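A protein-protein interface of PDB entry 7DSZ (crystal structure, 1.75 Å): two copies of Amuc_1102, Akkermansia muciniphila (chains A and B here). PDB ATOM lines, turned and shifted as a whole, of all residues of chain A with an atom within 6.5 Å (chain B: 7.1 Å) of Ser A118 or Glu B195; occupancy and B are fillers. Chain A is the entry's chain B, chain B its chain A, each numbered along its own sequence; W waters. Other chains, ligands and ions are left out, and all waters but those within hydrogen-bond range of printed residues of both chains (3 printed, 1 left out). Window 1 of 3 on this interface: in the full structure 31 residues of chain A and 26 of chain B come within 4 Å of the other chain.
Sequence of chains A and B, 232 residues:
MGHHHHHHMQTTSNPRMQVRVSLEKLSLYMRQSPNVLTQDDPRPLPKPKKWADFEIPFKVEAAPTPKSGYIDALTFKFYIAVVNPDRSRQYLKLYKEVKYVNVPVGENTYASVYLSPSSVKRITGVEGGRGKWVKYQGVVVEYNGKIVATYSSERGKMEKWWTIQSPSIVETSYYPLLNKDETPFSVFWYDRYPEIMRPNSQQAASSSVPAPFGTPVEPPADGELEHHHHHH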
ATOM      1  N   LYS A  49      -4.610   7.923 -14.890  1.00  0.00           N
ATOM      2  CA  LYS A  49      -4.061   8.920 -13.988  1.00  0.00           C
ATOM      3  C   LYS A  49      -3.605  10.144 -14.779  1.00  0.00           C
ATOM      4  O   LYS A  49      -3.500  10.118 -16.006  1.00  0.00           O
ATOM      5  CB  LYS A  49      -2.914   8.331 -13.178  1.00  0.00           C
ATOM      6  CG  LYS A  49      -3.366   7.228 -12.240  1.00  0.00           C
ATOM      7  CD  LYS A  49      -2.262   6.847 -11.289  1.00  0.00           C
ATOM      8  CE  LYS A  49      -1.038   6.370 -12.046  1.00  0.00           C
ATOM      9  NZ  LYS A  49      -0.201   5.461 -11.194  1.00  0.00           N
ATOM     10  N   LYS A  50      -3.335  11.229 -14.056  1.00  0.00           N
ATOM     11  CA  LYS A  50      -3.100  12.539 -14.650  1.00  0.00           C
ATOM     12  C   LYS A  50      -1.617  12.887 -14.593  1.00  0.00           C
ATOM     13  O   LYS A  50      -1.037  12.979 -13.505  1.00  0.00           O
ATOM     14  CB  LYS A  50      -3.923  13.605 -13.928  1.00  0.00           C
ATOM     15  CG  LYS A  50      -5.391  13.658 -14.340  1.00  0.00           C
ATOM     16  CD  LYS A  50      -5.537  14.229 -15.743  1.00  0.00           C
ATOM     17  CE  LYS A  50      -6.902  14.869 -15.957  1.00  0.00           C
ATOM     18  NZ  LYS A  50      -6.952  15.595 -17.266  1.00  0.00           N
ATOM     19  N   TRP A  51      -1.015  13.086 -15.763  1.00  0.00           N
ATOM     20  CA  TRP A  51       0.368  13.530 -15.883  1.00  0.00           C
ATOM     21  C   TRP A  51       0.433  15.051 -15.939  1.00  0.00           C
ATOM     22  O   TRP A  51      -0.465  15.703 -16.472  1.00  0.00           O
ATOM     23  CB  TRP A  51       1.008  12.965 -17.155  1.00  0.00           C
ATOM     24  CG  TRP A  51       1.309  11.508 -17.069  1.00  0.00           C
ATOM     25  CD1 TRP A  51       0.409  10.482 -17.076  1.00  0.00           C
ATOM     26  CD2 TRP A  51       2.610  10.905 -16.982  1.00  0.00           C
ATOM     27  NE1 TRP A  51       1.072   9.272 -16.992  1.00  0.00           N
ATOM     28  CE2 TRP A  51       2.421   9.508 -16.934  1.00  0.00           C
ATOM     29  CE3 TRP A  51       3.912  11.413 -16.933  1.00  0.00           C
ATOM     30  CZ2 TRP A  51       3.485   8.615 -16.828  1.00  0.00           C
ATOM     31  CZ3 TRP A  51       4.966  10.525 -16.839  1.00  0.00           C
ATOM     32  CH2 TRP A  51       4.744   9.137 -16.787  1.00  0.00           C
ATOM     33  N   LEU A 115       5.995  15.534 -15.404  1.00  0.00           N
ATOM     34  CA  LEU A 115       6.055  14.892 -14.095  1.00  0.00           C
ATOM     35  C   LEU A 115       5.015  13.784 -14.039  1.00  0.00           C
ATOM     36  O   LEU A 115       3.901  13.940 -14.553  1.00  0.00           O
ATOM     37  CB  LEU A 115       5.796  15.890 -12.956  1.00  0.00           C
ATOM     38  CG  LEU A 115       6.933  16.801 -12.534  1.00  0.00           C
ATOM     39  CD1 LEU A 115       6.406  17.794 -11.476  1.00  0.00           C
ATOM     40  CD2 LEU A 115       8.094  15.980 -11.981  1.00  0.00           C
ATOM     41  N   SER A 116       5.377  12.664 -13.408  1.00  0.00           N
ATOM     42  CA  SER A 116       4.513  11.500 -13.366  1.00  0.00           C
ATOM     43  C   SER A 116       3.296  11.758 -12.477  1.00  0.00           C
ATOM     44  O   SER A 116       3.301  12.675 -11.653  1.00  0.00           O
ATOM     45  CB  SER A 116       5.278  10.306 -12.809  1.00  0.00           C
ATOM     46  OG  SER A 116       5.536  10.566 -11.436  1.00  0.00           O
ATOM     47  N   PRO A 117       2.256  10.929 -12.599  1.00  0.00           N
ATOM     48  CA  PRO A 117       1.103  11.087 -11.690  1.00  0.00           C
ATOM     49  C   PRO A 117       1.482  10.937 -10.226  1.00  0.00           C
ATOM     50  O   PRO A 117       0.957  11.667  -9.376  1.00  0.00           O
ATOM     51  CB  PRO A 117       0.137   9.992 -12.167  1.00  0.00           C
ATOM     52  CG  PRO A 117       0.485   9.807 -13.638  1.00  0.00           C
ATOM     53  CD  PRO A 117       1.994   9.953 -13.671  1.00  0.00           C
ATOM     54  N   SER A 118       2.412  10.034  -9.902  1.00  0.00           N
ATOM     55  CA  SER A 118       2.792   9.866  -8.501  1.00  0.00           C
ATOM     56  C   SER A 118       3.614  11.046  -7.994  1.00  0.00           C
ATOM     57  O   SER A 118       3.538  11.393  -6.808  1.00  0.00           O
ATOM     58  CB  SER A 118       3.546   8.547  -8.307  1.00  0.00           C
ATOM     59  OG  SER A 118       4.814   8.544  -8.947  1.00  0.00           O
ATOM     60  N   SER A 119       4.398  11.690  -8.863  1.00  0.00           N
ATOM     61  CA  SER A 119       5.073  12.916  -8.449  1.00  0.00           C
ATOM     62  C   SER A 119       4.055  13.998  -8.113  1.00  0.00           C
ATOM     63  O   SER A 119       4.157  14.660  -7.072  1.00  0.00           O
ATOM     64  CB  SER A 119       6.030  13.405  -9.546  1.00  0.00           C
ATOM     65  OG  SER A 119       7.250  12.676  -9.534  1.00  0.00           O
ATOM     66  N   VAL A 120       3.058  14.184  -8.982  1.00  0.00           N
ATOM     67  CA  VAL A 120       2.034  15.200  -8.747  1.00  0.00           C
ATOM     68  C   VAL A 120       1.247  14.882  -7.481  1.00  0.00           C
ATOM     69  O   VAL A 120       0.967  15.772  -6.666  1.00  0.00           O
ATOM     70  CB  VAL A 120       1.103  15.326  -9.964  1.00  0.00           C
ATOM     71  CG1 VAL A 120      -0.055  16.293  -9.650  1.00  0.00           C
ATOM     72  CG2 VAL A 120       1.867  15.824 -11.177  1.00  0.00           C
ATOM     73  N   LYS A 121       0.869  13.613  -7.297  1.00  0.00           N
ATOM     74  CA  LYS A 121       0.080  13.258  -6.115  1.00  0.00           C
ATOM     75  C   LYS A 121       0.891  13.428  -4.838  1.00  0.00           C
ATOM     76  O   LYS A 121       0.364  13.896  -3.816  1.00  0.00           O
ATOM     77  CB  LYS A 121      -0.443  11.827  -6.225  1.00  0.00           C
ATOM     78  CG  LYS A 121      -1.234  11.358  -4.984  1.00  0.00           C
ATOM     79  CD  LYS A 121      -2.262  10.297  -5.378  1.00  0.00           C
ATOM     80  CE  LYS A 121      -3.010   9.728  -4.167  1.00  0.00           C
ATOM     81  NZ  LYS A 121      -2.242   8.624  -3.517  1.00  0.00           N
ATOM     82  N   ARG A 122       2.171  13.060  -4.871  1.00  0.00           N
ATOM     83  CA  ARG A 122       3.016  13.249  -3.701  1.00  0.00           C
ATOM     84  C   ARG A 122       3.171  14.730  -3.376  1.00  0.00           C
ATOM     85  O   ARG A 122       3.077  15.131  -2.210  1.00  0.00           O
ATOM     86  CB  ARG A 122       4.376  12.596  -3.925  1.00  0.00           C
ATOM     87  CG  ARG A 122       5.293  12.678  -2.731  1.00  0.00           C
ATOM     88  CD  ARG A 122       6.606  11.960  -2.969  1.00  0.00           C
ATOM     89  NE  ARG A 122       7.428  11.993  -1.766  1.00  0.00           N
ATOM     90  CZ  ARG A 122       8.742  11.821  -1.743  1.00  0.00           C
ATOM     91  NH1 ARG A 122       9.411  11.584  -2.874  1.00  0.00           N
ATOM     92  NH2 ARG A 122       9.388  11.891  -0.585  1.00  0.00           N
ATOM     93  N   ILE A 123       3.381  15.564  -4.399  1.00  0.00           N
ATOM     94  CA  ILE A 123       3.618  16.985  -4.155  1.00  0.00           C
ATOM     95  C   ILE A 123       2.375  17.650  -3.585  1.00  0.00           C
ATOM     96  O   ILE A 123       2.462  18.464  -2.657  1.00  0.00           O
ATOM     97  CB  ILE A 123       4.063  17.688  -5.449  1.00  0.00           C
ATOM     98  CG1 ILE A 123       5.485  17.281  -5.830  1.00  0.00           C
ATOM     99  CG2 ILE A 123       3.959  19.216  -5.311  1.00  0.00           C
ATOM    100  CD1 ILE A 123       5.793  17.612  -7.267  1.00  0.00           C
ATOM    101  N   GLU A 127      -4.600  13.150  -6.545  1.00  0.00           N
ATOM    102  CA  GLU A 127      -4.376  12.782  -7.935  1.00  0.00           C
ATOM    103  C   GLU A 127      -4.849  13.918  -8.837  1.00  0.00           C
ATOM    104  O   GLU A 127      -5.933  14.474  -8.636  1.00  0.00           O
ATOM    105  CB  GLU A 127      -5.111  11.479  -8.256  1.00  0.00           C
ATOM    106  CG  GLU A 127      -4.758  10.849  -9.598  1.00  0.00           C
ATOM    107  CD  GLU A 127      -3.301  10.378  -9.694  1.00  0.00           C
ATOM    108  OE1 GLU A 127      -2.732   9.866  -8.697  1.00  0.00           O
ATOM    109  OE2 GLU A 127      -2.724  10.515 -10.791  1.00  0.00           O
ATOM    110  N   TYR A 175      11.424  13.159  -7.533  1.00  0.00           N
ATOM    111  CA  TYR A 175      10.369  13.776  -8.329  1.00  0.00           C
ATOM    112  C   TYR A 175      10.904  14.019  -9.744  1.00  0.00           C
ATOM    113  O   TYR A 175      10.964  15.165 -10.199  1.00  0.00           O
ATOM    114  CB  TYR A 175       9.888  15.083  -7.715  1.00  0.00           C
ATOM    115  CG  TYR A 175       9.424  15.005  -6.276  1.00  0.00           C
ATOM    116  CD1 TYR A 175      10.337  15.071  -5.229  1.00  0.00           C
ATOM    117  CD2 TYR A 175       8.075  14.887  -5.974  1.00  0.00           C
ATOM    118  CE1 TYR A 175       9.924  15.013  -3.919  1.00  0.00           C
ATOM    119  CE2 TYR A 175       7.648  14.833  -4.658  1.00  0.00           C
ATOM    120  CZ  TYR A 175       8.585  14.902  -3.640  1.00  0.00           C
ATOM    121  OH  TYR A 175       8.188  14.851  -2.329  1.00  0.00           O
ATOM    122  N   PRO A 176      11.342  12.975 -10.445  1.00  0.00           N
ATOM    123  CA  PRO A 176      12.134  13.200 -11.666  1.00  0.00           C
ATOM    124  C   PRO A 176      11.307  13.837 -12.782  1.00  0.00           C
ATOM    125  O   PRO A 176      10.184  13.417 -13.077  1.00  0.00           O
ATOM    126  CB  PRO A 176      12.621  11.792 -12.048  1.00  0.00           C
ATOM    127  CG  PRO A 176      11.666  10.861 -11.397  1.00  0.00           C
ATOM    128  CD  PRO A 176      11.170  11.544 -10.138  1.00  0.00           C
ATOM    129  N   LEU A 178      10.738  14.293 -16.676  1.00  0.00           N
ATOM    130  CA  LEU A 178      10.850  13.283 -17.709  1.00  0.00           C
ATOM    131  C   LEU A 178      10.694  13.940 -19.068  1.00  0.00           C
ATOM    132  O   LEU A 178       9.837  14.812 -19.239  1.00  0.00           O
ATOM    133  CB  LEU A 178       9.775  12.226 -17.509  1.00  0.00           C
ATOM    134  CG  LEU A 178       9.848  11.515 -16.147  1.00  0.00           C
ATOM    135  CD1 LEU A 178       8.578  10.704 -15.901  1.00  0.00           C
ATOM    136  CD2 LEU A 178      11.056  10.609 -16.120  1.00  0.00           C
ATOM    137  N   TYR B  70       4.506   9.247   0.831  1.00  0.00           N
ATOM    138  CA  TYR B  70       5.433   8.532  -0.030  1.00  0.00           C
ATOM    139  C   TYR B  70       6.836   8.639   0.544  1.00  0.00           C
ATOM    140  O   TYR B  70       7.147   9.559   1.309  1.00  0.00           O
ATOM    141  CB  TYR B  70       5.466   9.112  -1.454  1.00  0.00           C
ATOM    142  CG  TYR B  70       4.219   8.960  -2.282  1.00  0.00           C
ATOM    143  CD1 TYR B  70       3.127   9.808  -2.103  1.00  0.00           C
ATOM    144  CD2 TYR B  70       4.150   8.000  -3.287  1.00  0.00           C
ATOM    145  CE1 TYR B  70       1.990   9.682  -2.885  1.00  0.00           C
ATOM    146  CE2 TYR B  70       3.025   7.870  -4.070  1.00  0.00           C
ATOM    147  CZ  TYR B  70       1.949   8.715  -3.869  1.00  0.00           C
ATOM    148  OH  TYR B  70       0.832   8.576  -4.655  1.00  0.00           O
ATOM    149  N   LEU B  74      13.029   3.204  -3.432  1.00  0.00           N
ATOM    150  CA  LEU B  74      13.504   1.906  -2.972  1.00  0.00           C
ATOM    151  C   LEU B  74      14.279   1.260  -4.111  1.00  0.00           C
ATOM    152  O   LEU B  74      13.865   1.352  -5.267  1.00  0.00           O
ATOM    153  CB  LEU B  74      12.357   0.958  -2.584  1.00  0.00           C
ATOM    154  CG  LEU B  74      11.590   1.241  -1.296  1.00  0.00           C
ATOM    155  CD1 LEU B  74      10.397   0.299  -1.167  1.00  0.00           C
ATOM    156  CD2 LEU B  74      12.525   1.122  -0.115  1.00  0.00           C
ATOM    157  N   VAL B  98      16.398  -2.584  -9.961  1.00  0.00           N
ATOM    158  CA  VAL B  98      15.282  -1.722 -10.348  1.00  0.00           C
ATOM    159  C   VAL B  98      15.073  -0.709  -9.235  1.00  0.00           C
ATOM    160  O   VAL B  98      14.733  -1.085  -8.104  1.00  0.00           O
ATOM    161  CB  VAL B  98      13.993  -2.518 -10.605  1.00  0.00           C
ATOM    162  CG1 VAL B  98      12.834  -1.576 -11.034  1.00  0.00           C
ATOM    163  CG2 VAL B  98      14.231  -3.604 -11.656  1.00  0.00           C
ATOM    164  N   LYS B  99      15.271   0.570  -9.544  1.00  0.00           N
ATOM    165  CA  LYS B  99      15.055   1.633  -8.571  1.00  0.00           C
ATOM    166  C   LYS B  99      13.670   2.235  -8.790  1.00  0.00           C
ATOM    167  O   LYS B  99      13.392   2.791  -9.857  1.00  0.00           O
ATOM    168  CB  LYS B  99      16.136   2.706  -8.678  1.00  0.00           C
ATOM    169  CG  LYS B  99      15.942   3.844  -7.669  1.00  0.00           C
ATOM    170  CD  LYS B  99      17.230   4.639  -7.487  1.00  0.00           C
ATOM    171  CE  LYS B  99      17.057   5.706  -6.412  1.00  0.00           C
ATOM    172  NZ  LYS B  99      18.221   5.809  -5.481  1.00  0.00           N
ATOM    173  N   TYR B 100      12.805   2.119  -7.783  1.00  0.00           N
ATOM    174  CA  TYR B 100      11.478   2.720  -7.826  1.00  0.00           C
ATOM    175  C   TYR B 100      11.503   4.071  -7.126  1.00  0.00           C
ATOM    176  O   TYR B 100      12.251   4.273  -6.167  1.00  0.00           O
ATOM    177  CB  TYR B 100      10.432   1.813  -7.166  1.00  0.00           C
ATOM    178  CG  TYR B 100      10.185   0.533  -7.934  1.00  0.00           C
ATOM    179  CD1 TYR B 100       9.385   0.530  -9.070  1.00  0.00           C
ATOM    180  CD2 TYR B 100      10.756  -0.667  -7.530  1.00  0.00           C
ATOM    181  CE1 TYR B 100       9.163  -0.641  -9.786  1.00  0.00           C
ATOM    182  CE2 TYR B 100      10.543  -1.842  -8.243  1.00  0.00           C
ATOM    183  CZ  TYR B 100       9.745  -1.817  -9.363  1.00  0.00           C
ATOM    184  OH  TYR B 100       9.512  -2.967 -10.068  1.00  0.00           O
ATOM    185  N   VAL B 101      10.687   5.005  -7.614  1.00  0.00           N
ATOM    186  CA  VAL B 101      10.610   6.332  -7.018  1.00  0.00           C
ATOM    187  C   VAL B 101       9.164   6.649  -6.674  1.00  0.00           C
ATOM    188  O   VAL B 101       8.231   6.139  -7.299  1.00  0.00           O
ATOM    189  CB  VAL B 101      11.204   7.423  -7.938  1.00  0.00           C
ATOM    190  CG1 VAL B 101      12.713   7.278  -8.015  1.00  0.00           C
ATOM    191  CG2 VAL B 101      10.571   7.377  -9.332  1.00  0.00           C
ATOM    192  N   ASN B 102       8.982   7.529  -5.687  1.00  0.00           N
ATOM    193  CA  ASN B 102       7.657   7.865  -5.170  1.00  0.00           C
ATOM    194  C   ASN B 102       6.907   6.599  -4.774  1.00  0.00           C
ATOM    195  O   ASN B 102       5.861   6.266  -5.330  1.00  0.00           O
ATOM    196  CB  ASN B 102       6.830   8.661  -6.188  1.00  0.00           C
ATOM    197  CG  ASN B 102       7.489   9.956  -6.597  1.00  0.00           C
ATOM    198  OD1 ASN B 102       8.194  10.601  -5.808  1.00  0.00           O
ATOM    199  ND2 ASN B 102       7.268  10.350  -7.851  1.00  0.00           N
ATOM    200  N   VAL B 103       7.461   5.867  -3.815  1.00  0.00           N
ATOM    201  CA  VAL B 103       6.869   4.609  -3.368  1.00  0.00           C
ATOM    202  C   VAL B 103       5.850   4.940  -2.282  1.00  0.00           C
ATOM    203  O   VAL B 103       6.225   5.552  -1.269  1.00  0.00           O
ATOM    204  CB  VAL B 103       7.922   3.625  -2.854  1.00  0.00           C
ATOM    205  CG1 VAL B 103       7.261   2.297  -2.497  1.00  0.00           C
ATOM    206  CG2 VAL B 103       9.027   3.410  -3.907  1.00  0.00           C
ATOM    207  N   PRO B 104       4.582   4.585  -2.455  1.00  0.00           N
ATOM    208  CA  PRO B 104       3.575   4.970  -1.465  1.00  0.00           C
ATOM    209  C   PRO B 104       3.760   4.178  -0.181  1.00  0.00           C
ATOM    210  O   PRO B 104       4.296   3.067  -0.177  1.00  0.00           O
ATOM    211  CB  PRO B 104       2.254   4.625  -2.156  1.00  0.00           C
ATOM    212  CG  PRO B 104       2.608   3.493  -3.062  1.00  0.00           C
ATOM    213  CD  PRO B 104       3.995   3.800  -3.556  1.00  0.00           C
ATOM    214  N   ASP B 181       9.837  -0.952 -17.905  1.00  0.00           N
ATOM    215  CA  ASP B 181       9.924   0.041 -18.964  1.00  0.00           C
ATOM    216  C   ASP B 181      10.861  -0.380 -20.087  1.00  0.00           C
ATOM    217  O   ASP B 181      10.950   0.329 -21.098  1.00  0.00           O
ATOM    218  CB  ASP B 181      10.351   1.392 -18.379  1.00  0.00           C
ATOM    219  CG  ASP B 181       9.224   2.053 -17.585  1.00  0.00           C
ATOM    220  OD1 ASP B 181       8.023   1.765 -17.851  1.00  0.00           O
ATOM    221  OD2 ASP B 181       9.539   2.841 -16.684  1.00  0.00           O
ATOM    222  N   TYR B 190      -0.402   0.335 -15.278  1.00  0.00           N
ATOM    223  CA  TYR B 190       0.452   1.347 -14.677  1.00  0.00           C
ATOM    224  C   TYR B 190       0.170   1.509 -13.187  1.00  0.00           C
ATOM    225  O   TYR B 190       1.088   1.821 -12.420  1.00  0.00           O
ATOM    226  CB  TYR B 190       0.323   2.686 -15.419  1.00  0.00           C
ATOM    227  CG  TYR B 190      -1.043   3.024 -15.982  1.00  0.00           C
ATOM    228  CD1 TYR B 190      -2.005   3.659 -15.200  1.00  0.00           C
ATOM    229  CD2 TYR B 190      -1.353   2.763 -17.315  1.00  0.00           C
ATOM    230  CE1 TYR B 190      -3.246   3.987 -15.717  1.00  0.00           C
ATOM    231  CE2 TYR B 190      -2.593   3.094 -17.840  1.00  0.00           C
ATOM    232  CZ  TYR B 190      -3.533   3.702 -17.033  1.00  0.00           C
ATOM    233  OH  TYR B 190      -4.765   4.031 -17.548  1.00  0.00           O
ATOM    234  N   TYR B 193       2.280  -0.919 -10.142  1.00  0.00           N
ATOM    235  CA  TYR B 193       3.660  -0.779  -9.706  1.00  0.00           C
ATOM    236  C   TYR B 193       3.976   0.688  -9.466  1.00  0.00           C
ATOM    237  O   TYR B 193       3.305   1.569 -10.020  1.00  0.00           O
ATOM    238  CB  TYR B 193       4.646  -1.325 -10.756  1.00  0.00           C
ATOM    239  CG  TYR B 193       4.253  -2.624 -11.420  1.00  0.00           C
ATOM    240  CD1 TYR B 193       3.430  -2.634 -12.542  1.00  0.00           C
ATOM    241  CD2 TYR B 193       4.710  -3.843 -10.933  1.00  0.00           C
ATOM    242  CE1 TYR B 193       3.070  -3.824 -13.166  1.00  0.00           C
ATOM    243  CE2 TYR B 193       4.368  -5.037 -11.560  1.00  0.00           C
ATOM    244  CZ  TYR B 193       3.557  -5.026 -12.670  1.00  0.00           C
ATOM    245  OH  TYR B 193       3.206  -6.216 -13.276  1.00  0.00           O
ATOM    246  N   PRO B 194       5.001   0.990  -8.667  1.00  0.00           N
ATOM    247  CA  PRO B 194       5.491   2.372  -8.599  1.00  0.00           C
ATOM    248  C   PRO B 194       6.242   2.739  -9.872  1.00  0.00           C
ATOM    249  O   PRO B 194       6.584   1.893 -10.702  1.00  0.00           O
ATOM    250  CB  PRO B 194       6.436   2.385  -7.396  1.00  0.00           C
ATOM    251  CG  PRO B 194       6.260   1.017  -6.732  1.00  0.00           C
ATOM    252  CD  PRO B 194       5.788   0.098  -7.802  1.00  0.00           C
ATOM    253  N   GLU B 195       6.505   4.036  -9.997  1.00  0.00           N
ATOM    254  CA  GLU B 195       7.322   4.566 -11.082  1.00  0.00           C
ATOM    255  C   GLU B 195       8.761   4.056 -10.979  1.00  0.00           C
ATOM    256  O   GLU B 195       9.314   3.915  -9.885  1.00  0.00           O
ATOM    257  CB  GLU B 195       7.280   6.104 -11.027  1.00  0.00           C
ATOM    258  CG  GLU B 195       8.212   6.830 -11.997  1.00  0.00           C
ATOM    259  CD  GLU B 195       8.136   8.344 -11.794  1.00  0.00           C
ATOM    260  OE1 GLU B 195       7.350   8.781 -10.919  1.00  0.00           O
ATOM    261  OE2 GLU B 195       8.852   9.078 -12.509  1.00  0.00           O
ATOM    262  N   ILE B 196       9.374   3.767 -12.131  1.00  0.00           N
ATOM    263  CA  ILE B 196      10.754   3.294 -12.199  1.00  0.00           C
ATOM    264  C   ILE B 196      11.660   4.466 -12.543  1.00  0.00           C
ATOM    265  O   ILE B 196      11.388   5.201 -13.500  1.00  0.00           O
ATOM    266  CB  ILE B 196      10.910   2.176 -13.248  1.00  0.00           C
ATOM    267  CG1 ILE B 196      10.056   0.957 -12.890  1.00  0.00           C
ATOM    268  CG2 ILE B 196      12.399   1.791 -13.418  1.00  0.00           C
ATOM    269  CD1 ILE B 196       9.961  -0.083 -14.015  1.00  0.00           C
ATOM    270  N   MET B 197      12.756   4.618 -11.797  1.00  0.00           N
ATOM    271  CA  MET B 197      13.707   5.682 -12.087  1.00  0.00           C
ATOM    272  C   MET B 197      14.512   5.336 -13.336  1.00  0.00           C
ATOM    273  O   MET B 197      15.079   4.246 -13.433  1.00  0.00           O
ATOM    274  CB  MET B 197      14.649   5.892 -10.909  1.00  0.00           C
ATOM    275  CG  MET B 197      15.775   6.825 -11.242  1.00  0.00           C
ATOM    276  SD  MET B 197      15.311   8.495 -10.800  1.00  0.00           S
ATOM    277  CE  MET B 197      15.826   8.479  -9.077  1.00  0.00           C
ATOM    278  N   ARG B 198      14.563   6.265 -14.288  1.00  0.00           N
ATOM    279  CA  ARG B 198      15.247   6.034 -15.560  1.00  0.00           C
ATOM    280  C   ARG B 198      16.762   6.013 -15.349  1.00  0.00           C
ATOM    281  O   ARG B 198      17.253   6.446 -14.306  1.00  0.00           O
ATOM    282  CB  ARG B 198      14.866   7.123 -16.567  1.00  0.00           C
ATOM    283  CG  ARG B 198      13.391   7.156 -16.948  1.00  0.00           C
ATOM    284  CD  ARG B 198      13.114   6.261 -18.141  1.00  0.00           C
ATOM    285  NE  ARG B 198      11.682   6.066 -18.356  1.00  0.00           N
ATOM    286  CZ  ARG B 198      11.171   5.453 -19.421  1.00  0.00           C
ATOM    287  NH1 ARG B 198      11.976   4.984 -20.364  1.00  0.00           N
ATOM    288  NH2 ARG B 198       9.856   5.311 -19.548  1.00  0.00           N
HETATM  289  O   HOH W   1       5.262   5.833  -8.080  1.00  0.00           O
HETATM  290  O   HOH W   2      10.992  10.556  -5.858  1.00  0.00           O
HETATM  291  O   HOH W   3       8.110  12.096 -12.103  1.00  0.00           O
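The side-chain hydroxyl (OG) of Ser A118 sits at hydrogen-bond distance from the side-chain carboxylate (OE1) of Glu B195.
The side-chain amide nitrogen (ND2) of Asn B102 sits at hydrogen-bond distance from the side-chain hydroxyl (OG) of Ser A118 (3.2 Å).
The side-chain carboxylate (OE1) of Glu B195 lies within hydrogen-bond range of the side-chain hydroxyl (OG) of Ser A116, 2.6 Å away.
The side-chain hydroxyl of Tyr B70 is in hydrogen-bond range of the side-chain amino group of Lys A121, 3.3 Å away.
OD1 of Asn B102 lies within hydrogen-bond range of NH1 of Arg A122, at 3.3 Å.
ND2 of Asn B102 is in hydrogen-bond range of OG of Ser A119 (2.9 Å).
The side-chain hydroxyl (OH) of Tyr A175 lies within hydrogen-bond range of the guanidinium group (NE) of Arg A122 (3.0 Å).
O of Glu B195 lies within hydrogen-bond range of N of Val B101 (2.9 Å).
ND2 of Asn B102 is in hydrogen-bond range of OE1 of Glu B195, at 3.4 Å.
The backbone NH of Ser A119 is in hydrogen-bond range of the side-chain hydroxyl of Ser A116, 3.0 Å away.
The side-chain hydroxyl (OG) of Ser A116 sits at hydrogen-bond distance from the side-chain hydroxyl (OG) of Ser A118, 3.3 Å away.
ND2 of Asn B102 touches OG of Ser A116, 3.99 Å away.
Arg A122 touches Tyr B70.
CG of Pro A176 touches OE2 of Glu B195, 3.5 Å away.
Leu A178 touches Glu B195.
Ser A118 touches two residues of chain B.
Printed residues of chain B within 4 Å of Ser A119: Asn B102 (2.9 Å).
Of the printed residues of chain B, Pro A176 touches Glu B195 (3.5 Å).
Tyr B190 touches none of the printed residues of chain A.
Glu B195 touches just these residues of chain A: Ser A116, Ser A118, Pro A176 and Leu A178.
The nearest residue of chain A that does not touch Glu B195 is Ser A119 (4.1 Å).
Of the 17 printed residues of chain B, 3 touch a printed residue of chain A.
Hydrophobic or aromatic side chains of chain B that line the printed part of chain A: Tyr B70.
Along chain B the printed residues that touch a printed residue of chain A span positions 70 to 195.
Hydrophobic or aromatic side chains of chain A within 4 Å of the printed part of chain B: Pro A176 and Leu A178.
Among the printed residues, 10 pairs touch across the chains.
Among the printed residues, no Asp or Glu carboxylate lies within 4 Å of a Lys or Arg side-chain nitrogen of the other chain.
No position is printed for both chains.
Of the 10 pairs that touch across the chains among the printed residues, none has its exchanged pair printed and touching as well.
Water W3 lies within hydrogen-bond range of the backbone carbonyl oxygen (O) of Pro A176 (2.6 Å), the side-chain hydroxyl (OG) of Ser A119 (2.8 Å), the side-chain hydroxyl (OG) of Ser A116 (3.1 Å) and the side-chain carboxylate (OE2) of Glu B195 (3.1 Å).
Water W2 bridges OD1 of Asn B102 (2.8 Å) and N of Tyr A175 (3.1 Å).
Water W1 lies within hydrogen-bond range of O of Asn B102 (2.8 Å), OG of Ser A118 (2.9 Å), N of Glu B195 (2.9 Å) and O of Val B101 (3.1 Å).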
